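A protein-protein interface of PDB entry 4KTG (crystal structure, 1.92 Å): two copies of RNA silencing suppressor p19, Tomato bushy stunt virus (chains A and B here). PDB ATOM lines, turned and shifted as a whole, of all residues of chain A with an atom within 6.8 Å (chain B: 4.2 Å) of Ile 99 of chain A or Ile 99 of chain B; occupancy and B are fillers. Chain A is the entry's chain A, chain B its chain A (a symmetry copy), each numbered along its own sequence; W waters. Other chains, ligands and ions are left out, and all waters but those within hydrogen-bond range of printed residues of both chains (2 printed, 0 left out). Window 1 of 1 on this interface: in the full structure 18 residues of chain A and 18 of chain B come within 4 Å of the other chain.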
ATOM      1  N   TYR A  90     -31.387   2.354   6.633  1.00  0.00           N
ATOM      2  CA  TYR A  90     -32.029   3.608   7.022  1.00  0.00           C
ATOM      3  C   TYR A  90     -31.000   4.699   6.891  1.00  0.00           C
ATOM      4  O   TYR A  90     -29.850   4.526   7.322  1.00  0.00           O
ATOM      5  CB  TYR A  90     -32.596   3.564   8.408  1.00  0.00           C
ATOM      6  CG  TYR A  90     -33.108   4.908   8.891  1.00  0.00           C
ATOM      7  CD1 TYR A  90     -34.358   5.399   8.461  1.00  0.00           C
ATOM      8  CD2 TYR A  90     -32.345   5.745   9.658  1.00  0.00           C
ATOM      9  CE1 TYR A  90     -34.813   6.656   8.801  1.00  0.00           C
ATOM     10  CE2 TYR A  90     -32.860   6.975  10.120  1.00  0.00           C
ATOM     11  CZ  TYR A  90     -34.071   7.456   9.627  1.00  0.00           C
ATOM     12  OH  TYR A  90     -34.581   8.628  10.044  1.00  0.00           O
ATOM     13  N   SER A  91     -31.349   5.802   6.247  1.00  0.00           N
ATOM     14  CA  SER A  91     -30.500   6.999   6.138  1.00  0.00           C
ATOM     15  C   SER A  91     -31.221   8.253   6.594  1.00  0.00           C
ATOM     16  O   SER A  91     -32.383   8.409   6.315  1.00  0.00           O
ATOM     17  CB  SER A  91     -30.147   7.217   4.721  1.00  0.00           C
ATOM     18  OG  SER A  91     -29.341   6.162   4.180  1.00  0.00           O
ATOM     19  N   ILE A  92     -30.510   9.152   7.236  1.00  0.00           N
ATOM     20  CA  ILE A  92     -31.016  10.430   7.624  1.00  0.00           C
ATOM     21  C   ILE A  92     -29.942  11.474   7.435  1.00  0.00           C
ATOM     22  O   ILE A  92     -28.785  11.207   7.706  1.00  0.00           O
ATOM     23  CB  ILE A  92     -31.531  10.431   9.042  1.00  0.00           C
ATOM     24  CG1 ILE A  92     -32.184  11.803   9.430  1.00  0.00           C
ATOM     25  CG2 ILE A  92     -30.487  10.054  10.100  1.00  0.00           C
ATOM     26  CD1 ILE A  92     -32.938  11.777  10.769  1.00  0.00           C
ATOM     27  N   ARG A  93     -30.306  12.666   6.968  1.00  0.00           N
ATOM     28  CA  ARG A  93     -29.393  13.754   6.860  1.00  0.00           C
ATOM     29  C   ARG A  93     -29.960  15.059   7.407  1.00  0.00           C
ATOM     30  O   ARG A  93     -31.115  15.414   7.077  1.00  0.00           O
ATOM     31  CB  ARG A  93     -29.028  13.878   5.435  1.00  0.00           C
ATOM     32  CG  ARG A  93     -28.134  15.057   5.277  1.00  0.00           C
ATOM     33  CD  ARG A  93     -27.545  15.194   3.917  1.00  0.00           C
ATOM     34  NE  ARG A  93     -26.405  16.086   4.091  1.00  0.00           N
ATOM     35  CZ  ARG A  93     -25.430  16.255   3.216  1.00  0.00           C
ATOM     36  NH1 ARG A  93     -25.416  15.603   2.024  1.00  0.00           N
ATOM     37  NH2 ARG A  93     -24.461  17.102   3.543  1.00  0.00           N
ATOM     38  N   PHE A  94     -29.180  15.790   8.190  1.00  0.00           N
ATOM     39  CA  PHE A  94     -29.608  17.019   8.829  1.00  0.00           C
ATOM     40  C   PHE A  94     -28.373  17.819   9.159  1.00  0.00           C
ATOM     41  O   PHE A  94     -27.376  17.285   9.658  1.00  0.00           O
ATOM     42  CB  PHE A  94     -30.338  16.711  10.119  1.00  0.00           C
ATOM     43  CG  PHE A  94     -30.963  17.910  10.797  1.00  0.00           C
ATOM     44  CD1 PHE A  94     -31.820  18.735  10.109  1.00  0.00           C
ATOM     45  CD2 PHE A  94     -30.763  18.148  12.167  1.00  0.00           C
ATOM     46  CE1 PHE A  94     -32.419  19.788  10.736  1.00  0.00           C
ATOM     47  CE2 PHE A  94     -31.365  19.209  12.809  1.00  0.00           C
ATOM     48  CZ  PHE A  94     -32.212  20.050  12.085  1.00  0.00           C
ATOM     49  N   VAL A  97     -24.741  16.515   8.211  1.00  0.00           N
ATOM     50  CA  VAL A  97     -24.392  15.230   8.740  1.00  0.00           C
ATOM     51  C   VAL A  97     -25.372  14.192   8.249  1.00  0.00           C
ATOM     52  O   VAL A  97     -26.613  14.344   8.447  1.00  0.00           O
ATOM     53  CB  VAL A  97     -24.375  15.225  10.268  1.00  0.00           C
ATOM     54  CG1 VAL A  97     -24.008  13.848  10.821  1.00  0.00           C
ATOM     55  CG2 VAL A  97     -23.364  16.277  10.806  1.00  0.00           C
ATOM     56  N   SER A  98     -24.813  13.139   7.657  1.00  0.00           N
ATOM     57  CA  SER A  98     -25.535  11.902   7.216  1.00  0.00           C
ATOM     58  C   SER A  98     -25.229  10.698   8.082  1.00  0.00           C
ATOM     59  O   SER A  98     -24.102  10.510   8.464  1.00  0.00           O
ATOM     60  CB  SER A  98     -25.222  11.722   5.748  1.00  0.00           C
ATOM     61  OG  SER A  98     -25.449  10.366   5.422  1.00  0.00           O
ATOM     62  N   ILE A  99     -26.245   9.989   8.564  1.00  0.00           N
ATOM     63  CA  ILE A  99     -26.111   8.744   9.302  1.00  0.00           C
ATOM     64  C   ILE A  99     -26.840   7.688   8.563  1.00  0.00           C
ATOM     65  O   ILE A  99     -28.017   7.922   8.144  1.00  0.00           O
ATOM     66  CB  ILE A  99     -26.638   8.854  10.765  1.00  0.00           C
ATOM     67  CG1 ILE A  99     -25.925   9.982  11.463  1.00  0.00           C
ATOM     68  CG2 ILE A  99     -26.492   7.514  11.473  1.00  0.00           C
ATOM     69  CD1 ILE A  99     -26.419  10.195  12.894  1.00  0.00           C
ATOM     70  N   THR A 100     -26.146   6.564   8.300  1.00  0.00           N
ATOM     71  CA  THR A 100     -26.744   5.403   7.686  1.00  0.00           C
ATOM     72  C   THR A 100     -26.619   4.240   8.640  1.00  0.00           C
ATOM     73  O   THR A 100     -25.541   4.036   9.240  1.00  0.00           O
ATOM     74  CB  THR A 100     -26.112   5.128   6.316  1.00  0.00           C
ATOM     75  OG1 THR A 100     -26.302   6.295   5.446  1.00  0.00           O
ATOM     76  CG2 THR A 100     -26.751   3.984   5.685  1.00  0.00           C
ATOM     77  N   VAL A 101     -27.712   3.534   8.827  1.00  0.00           N
ATOM     78  CA  VAL A 101     -27.846   2.311   9.640  1.00  0.00           C
ATOM     79  C   VAL A 101     -28.179   1.183   8.703  1.00  0.00           C
ATOM     80  O   VAL A 101     -29.243   1.198   8.013  1.00  0.00           O
ATOM     81  CB  VAL A 101     -28.903   2.377  10.750  1.00  0.00           C
ATOM     82  CG1 VAL A 101     -28.915   1.065  11.567  1.00  0.00           C
ATOM     83  CG2 VAL A 101     -28.684   3.520  11.697  1.00  0.00           C
ATOM     84  N   SER A 102     -27.310   0.172   8.607  1.00  0.00           N
ATOM     85  CA  SER A 102     -27.512  -0.870   7.578  1.00  0.00           C
ATOM     86  C   SER A 102     -27.191  -2.284   8.032  1.00  0.00           C
ATOM     87  O   SER A 102     -26.313  -2.493   8.887  1.00  0.00           O
ATOM     88  CB  SER A 102     -26.727  -0.619   6.252  1.00  0.00           C
ATOM     89  OG  SER A 102     -25.375  -0.280   6.533  1.00  0.00           O
ATOM     90  N   MET A 114     -31.515   0.976  16.364  1.00  0.00           N
ATOM     91  CA  MET A 114     -30.411   1.936  16.181  1.00  0.00           C
ATOM     92  C   MET A 114     -30.858   3.095  15.296  1.00  0.00           C
ATOM     93  O   MET A 114     -30.383   4.234  15.487  1.00  0.00           O
ATOM     94  CB  MET A 114     -29.167   1.295  15.573  1.00  0.00           C
ATOM     95  CG  MET A 114     -28.553   0.159  16.433  1.00  0.00           C
ATOM     96  SD  MET A 114     -28.112   0.829  18.047  1.00  0.00           S
ATOM     97  CE  MET A 114     -27.262   2.319  17.661  1.00  0.00           C
ATOM     98  N   ALA A 115     -31.736   2.836  14.325  1.00  0.00           N
ATOM     99  CA  ALA A 115     -32.190   3.943  13.417  1.00  0.00           C
ATOM    100  C   ALA A 115     -32.956   5.013  14.204  1.00  0.00           C
ATOM    101  O   ALA A 115     -32.704   6.171  14.030  1.00  0.00           O
ATOM    102  CB  ALA A 115     -33.071   3.390  12.262  1.00  0.00           C
ATOM    103  N   SER A 118     -30.557   6.932  16.322  1.00  0.00           N
ATOM    104  CA  SER A 118     -29.683   7.799  15.512  1.00  0.00           C
ATOM    105  C   SER A 118     -30.514   9.100  15.123  1.00  0.00           C
ATOM    106  O   SER A 118     -30.041  10.200  15.136  1.00  0.00           O
ATOM    107  CB  SER A 118     -29.316   7.082  14.247  1.00  0.00           C
ATOM    108  OG  SER A 118     -28.440   6.007  14.513  1.00  0.00           O
ATOM    109  N   LYS A 119     -31.765   8.870  14.722  1.00  0.00           N
ATOM    110  CA  LYS A 119     -32.648   9.964  14.328  1.00  0.00           C
ATOM    111  C   LYS A 119     -32.785  10.965  15.461  1.00  0.00           C
ATOM    112  O   LYS A 119     -32.588  12.117  15.282  1.00  0.00           O
ATOM    113  CB  LYS A 119     -34.012   9.369  13.896  1.00  0.00           C
ATOM    114  CG  LYS A 119     -35.052  10.456  13.487  1.00  0.00           C
ATOM    115  CD  LYS A 119     -36.292   9.704  13.015  1.00  0.00           C
ATOM    116  CE  LYS A 119     -37.328  10.656  12.416  1.00  0.00           C
ATOM    117  NZ  LYS A 119     -38.369   9.889  11.721  1.00  0.00           N
ATOM    118  N   GLU A 121     -30.956  11.487  18.111  1.00  0.00           N
ATOM    119  CA  GLU A 121     -29.687  12.165  18.436  1.00  0.00           C
ATOM    120  C   GLU A 121     -29.284  13.201  17.419  1.00  0.00           C
ATOM    121  O   GLU A 121     -28.854  14.327  17.797  1.00  0.00           O
ATOM    122  CB  GLU A 121     -28.522  11.152  18.717  1.00  0.00           C
ATOM    123  CG  GLU A 121     -28.904   9.955  19.646  1.00  0.00           C
ATOM    124  CD  GLU A 121     -28.353   9.974  21.091  1.00  0.00           C
ATOM    125  OE1 GLU A 121     -29.168  10.130  22.054  1.00  0.00           O
ATOM    126  OE2 GLU A 121     -27.111   9.858  21.274  1.00  0.00           O
ATOM    127  N   LEU A 122     -29.454  12.899  16.125  1.00  0.00           N
ATOM    128  CA  LEU A 122     -29.085  13.832  15.126  1.00  0.00           C
ATOM    129  C   LEU A 122     -30.015  15.103  15.175  1.00  0.00           C
ATOM    130  O   LEU A 122     -29.572  16.221  14.983  1.00  0.00           O
ATOM    131  CB  LEU A 122     -29.165  13.222  13.732  1.00  0.00           C
ATOM    132  CG  LEU A 122     -28.752  14.142  12.609  1.00  0.00           C
ATOM    133  CD1 LEU A 122     -27.378  14.781  12.733  1.00  0.00           C
ATOM    134  CD2 LEU A 122     -28.788  13.349  11.318  1.00  0.00           C
ATOM    135  N   TYR B  90     -16.994   8.149   9.488  1.00  0.00           N
ATOM    136  CA  TYR B  90     -16.762   7.190  10.567  1.00  0.00           C
ATOM    137  C   TYR B  90     -17.692   6.027  10.342  1.00  0.00           C
ATOM    138  O   TYR B  90     -18.880   6.228  10.045  1.00  0.00           O
ATOM    139  CB  TYR B  90     -16.962   7.787  11.926  1.00  0.00           C
ATOM    140  CG  TYR B  90     -16.898   6.766  13.046  1.00  0.00           C
ATOM    141  CD1 TYR B  90     -15.657   6.281  13.508  1.00  0.00           C
ATOM    142  CD2 TYR B  90     -18.022   6.188  13.571  1.00  0.00           C
ATOM    143  CE1 TYR B  90     -15.562   5.283  14.456  1.00  0.00           C
ATOM    144  CE2 TYR B  90     -17.934   5.266  14.635  1.00  0.00           C
ATOM    145  CZ  TYR B  90     -16.694   4.764  15.025  1.00  0.00           C
ATOM    146  OH  TYR B  90     -16.581   3.879  16.030  1.00  0.00           O
ATOM    147  N   SER B  91     -17.181   4.808  10.406  1.00  0.00           N
ATOM    148  CA  SER B  91     -17.977   3.572  10.327  1.00  0.00           C
ATOM    149  C   SER B  91     -17.711   2.647  11.498  1.00  0.00           C
ATOM    150  O   SER B  91     -16.587   2.518  11.914  1.00  0.00           O
ATOM    151  CB  SER B  91     -17.596   2.825   9.113  1.00  0.00           C
ATOM    152  OG  SER B  91     -17.912   3.528   7.903  1.00  0.00           O
ATOM    153  N   ILE B  92     -18.734   1.973  11.972  1.00  0.00           N
ATOM    154  CA  ILE B  92     -18.620   0.978  12.991  1.00  0.00           C
ATOM    155  C   ILE B  92     -19.555  -0.167  12.681  1.00  0.00           C
ATOM    156  O   ILE B  92     -20.660   0.062  12.220  1.00  0.00           O
ATOM    157  CB  ILE B  92     -18.886   1.539  14.365  1.00  0.00           C
ATOM    158  CG1 ILE B  92     -18.656   0.472  15.492  1.00  0.00           C
ATOM    159  CG2 ILE B  92     -20.275   2.165  14.542  1.00  0.00           C
ATOM    160  CD1 ILE B  92     -18.674   1.054  16.914  1.00  0.00           C
ATOM    161  N   SER B  98     -24.247  -2.147  10.893  1.00  0.00           N
ATOM    162  CA  SER B  98     -23.280  -1.086  10.461  1.00  0.00           C
ATOM    163  C   SER B  98     -23.856   0.312  10.557  1.00  0.00           C
ATOM    164  O   SER B  98     -24.997   0.510  10.228  1.00  0.00           O
ATOM    165  CB  SER B  98     -22.799  -1.479   9.083  1.00  0.00           C
ATOM    166  OG  SER B  98     -22.304  -0.316   8.452  1.00  0.00           O
ATOM    167  N   ILE B  99     -23.151   1.245  11.189  1.00  0.00           N
ATOM    168  CA  ILE B  99     -23.510   2.652  11.256  1.00  0.00           C
ATOM    169  C   ILE B  99     -22.407   3.438  10.657  1.00  0.00           C
ATOM    170  O   ILE B  99     -21.208   3.189  10.999  1.00  0.00           O
ATOM    171  CB  ILE B  99     -23.799   3.129  12.711  1.00  0.00           C
ATOM    172  CG1 ILE B  99     -24.874   2.262  13.311  1.00  0.00           C
ATOM    173  CG2 ILE B  99     -24.143   4.613  12.714  1.00  0.00           C
ATOM    174  CD1 ILE B  99     -25.185   2.630  14.762  1.00  0.00           C
ATOM    175  N   THR B 100     -22.759   4.317   9.699  1.00  0.00           N
ATOM    176  CA  THR B 100     -21.822   5.233   9.095  1.00  0.00           C
ATOM    177  C   THR B 100     -22.289   6.642   9.367  1.00  0.00           C
ATOM    178  O   THR B 100     -23.495   6.939   9.227  1.00  0.00           O
ATOM    179  CB  THR B 100     -21.653   4.931   7.601  1.00  0.00           C
ATOM    180  OG1 THR B 100     -21.173   3.554   7.431  1.00  0.00           O
ATOM    181  CG2 THR B 100     -20.673   5.829   7.011  1.00  0.00           C
ATOM    182  N   MET B 114     -21.607  12.943  16.723  1.00  0.00           N
ATOM    183  CA  MET B 114     -22.562  11.875  16.373  1.00  0.00           C
ATOM    184  C   MET B 114     -21.852  10.527  16.317  1.00  0.00           C
ATOM    185  O   MET B 114     -22.471   9.491  16.640  1.00  0.00           O
ATOM    186  CB  MET B 114     -23.264  12.126  15.042  1.00  0.00           C
ATOM    187  CG  MET B 114     -24.108  13.427  15.004  1.00  0.00           C
ATOM    188  SD  MET B 114     -25.360  13.343  16.296  1.00  0.00           S
ATOM    189  CE  MET B 114     -26.049  11.736  16.104  1.00  0.00           C
ATOM    190  N   SER B 118     -23.009   7.307  18.356  1.00  0.00           N
ATOM    191  CA  SER B 118     -23.443   6.124  17.592  1.00  0.00           C
ATOM    192  C   SER B 118     -22.665   4.861  18.170  1.00  0.00           C
ATOM    193  O   SER B 118     -23.190   3.797  18.339  1.00  0.00           O
ATOM    194  CB  SER B 118     -23.055   6.297  16.155  1.00  0.00           C
ATOM    195  OG  SER B 118     -23.834   7.301  15.540  1.00  0.00           O
ATOM    196  N   LEU B 122     -24.460   1.591  19.796  1.00  0.00           N
ATOM    197  CA  LEU B 122     -24.372   0.329  19.161  1.00  0.00           C
ATOM    198  C   LEU B 122     -23.724  -0.739  20.123  1.00  0.00           C
ATOM    199  O   LEU B 122     -24.122  -1.890  20.152  1.00  0.00           O
ATOM    200  CB  LEU B 122     -23.545   0.401  17.884  1.00  0.00           C
ATOM    201  CG  LEU B 122     -23.433  -0.898  17.124  1.00  0.00           C
ATOM    202  CD1 LEU B 122     -24.741  -1.585  16.765  1.00  0.00           C
ATOM    203  CD2 LEU B 122     -22.677  -0.624  15.839  1.00  0.00           C
HETATM  204  O   HOH W   1     -23.453   8.048   6.371  1.00  0.00           O
HETATM  205  O   HOH W   2     -24.263   1.975   7.368  1.00  0.00           O
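Printed residues of chain B within 4 Å of Thr 100 of chain A: Ser 98, Ile 99 and Thr 100. Of the printed residues of chain B, Ser 102 of chain A touches Ser 98. Ser 118 of chain A touches none of the printed residues of chain B. Of the printed residues of chain A, Ser 98 of chain B touches Thr 100, Val 101 and Ser 102. Of chain A, only Ile 99 (3.9 Å), Thr 100 (3.2 Å) and Met 114 (3.6 Å) come within 4 Å of Ile 99 of chain B. Of the printed residues of chain A, Thr 100 of chain B touches Ser 98 (3.7 Å), Ile 99 (3.2 Å) and Thr 100 (2.8 Å). Of the printed residues of chain A, Met 114 of chain B touches Ile 99, Glu 121 and Leu 122. The nearest printed residue of chain B that does not touch Ile 99 of chain A is Ser 118 of chain B (4.7 Å). The nearest printed residue of chain A that does not touch Met 114 of chain B is Val 97 of chain A (4.2 Å).
Ser 98 of chain A touches Thr 100 of chain B, and with the chains exchanged Thr 100 of chain A touches Ser 98 of chain B. Ile 99 of chain A touches Thr 100 of chain B, and with the chains exchanged Thr 100 of chain A touches Ile 99 of chain B. Ile 99 of chain A touches Met 114 of chain B, and with the chains exchanged Met 114 of chain A touches Ile 99 of chain B. Met 114 of chain A touches Leu 122 of chain B, and with the chains exchanged Leu 122 of chain A touches Met 114 of chain B.
Hydrophobic or aromatic side chains of chain B within 4 Å of the printed part of chain A: Ile 99 and Met 114. Hydrophobic or aromatic side chains of chain A within 4 Å of the printed part of chain B: Ile 99 and Met 114. Along chain A the printed residues that touch a printed residue of chain B span positions 98 to 122.
The backbone carbonyl oxygen (O) of Ile 99 of chain A sits at hydrogen-bond distance from the backbone NH (N) of Ile 92 of chain A, 2.9 Å away. The backbone carbonyl oxygen (O) of Tyr 90 of chain A lies within hydrogen-bond range of the backbone NH (N) of Val 101 of chain A (2.8 Å). N of Ile 92 of chain B is in hydrogen-bond range of O of Ile 99 of chain B, at 2.9 Å. OG of Ser 118 of chain B is in hydrogen-bond range of O of Met 114 of chain B. The side-chain hydroxyl (OG1) of Thr 100 of chain B sits at hydrogen-bond distance from the side-chain hydroxyl (OG) of Ser 91 of chain B (3.3 Å). O of Met 114 of chain A is in hydrogen-bond range of OG of Ser 118 of chain A (2.8 Å).
Ser 98 of chain A touches Thr 100 of chain B. Ile 99 of chain B touches Ile 99 of chain A (CG2 to CG2, 3.9 Å). Ile 99 of chain A touches Thr 100 of chain B. Met 114 of chain B touches Ile 99 of chain A. Ser 98 of chain B touches Thr 100 of chain A (O to O, 3.7 Å). O of Thr 100 of chain A touches CA of Ile 99 of chain B (3.2 Å). Val 101 of chain A touches Ser 98 of chain B (CA to O, 3.4 Å). Met 114 of chain A touches Ile 99 of chain B. Met 114 of chain A touches Leu 122 of chain B (CE to N, 3.6 Å). Glu 121 of chain A touches Met 114 of chain B (CB to CE, 3.6 Å).
N of Thr 100 of chain A is in hydrogen-bond range of O of Thr 100 of chain B, at 2.8 Å. N of Ser 102 of chain A sits at hydrogen-bond distance from O of Ser 98 of chain B (2.8 Å).
Water W2 lies within hydrogen-bond range of the side-chain hydroxyl (OG) of Ser 102 of chain A (2.6 Å), the backbone carbonyl oxygen (O) of Thr 100 of chain A (3.1 Å), the side-chain hydroxyl (OG) of Ser 98 of chain B (3.2 Å) and the side-chain hydroxyl (OG1) of Thr 100 of chain B (3.5 Å). Water W1 lies within hydrogen-bond range of the backbone carbonyl oxygen (O) of Thr 100 of chain B (3.1 Å), the side-chain hydroxyl (OG) of Ser 98 of chain A (3.2 Å) and the side-chain hydroxyl (OG1) of Thr 100 of chain A (3.5 Å).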
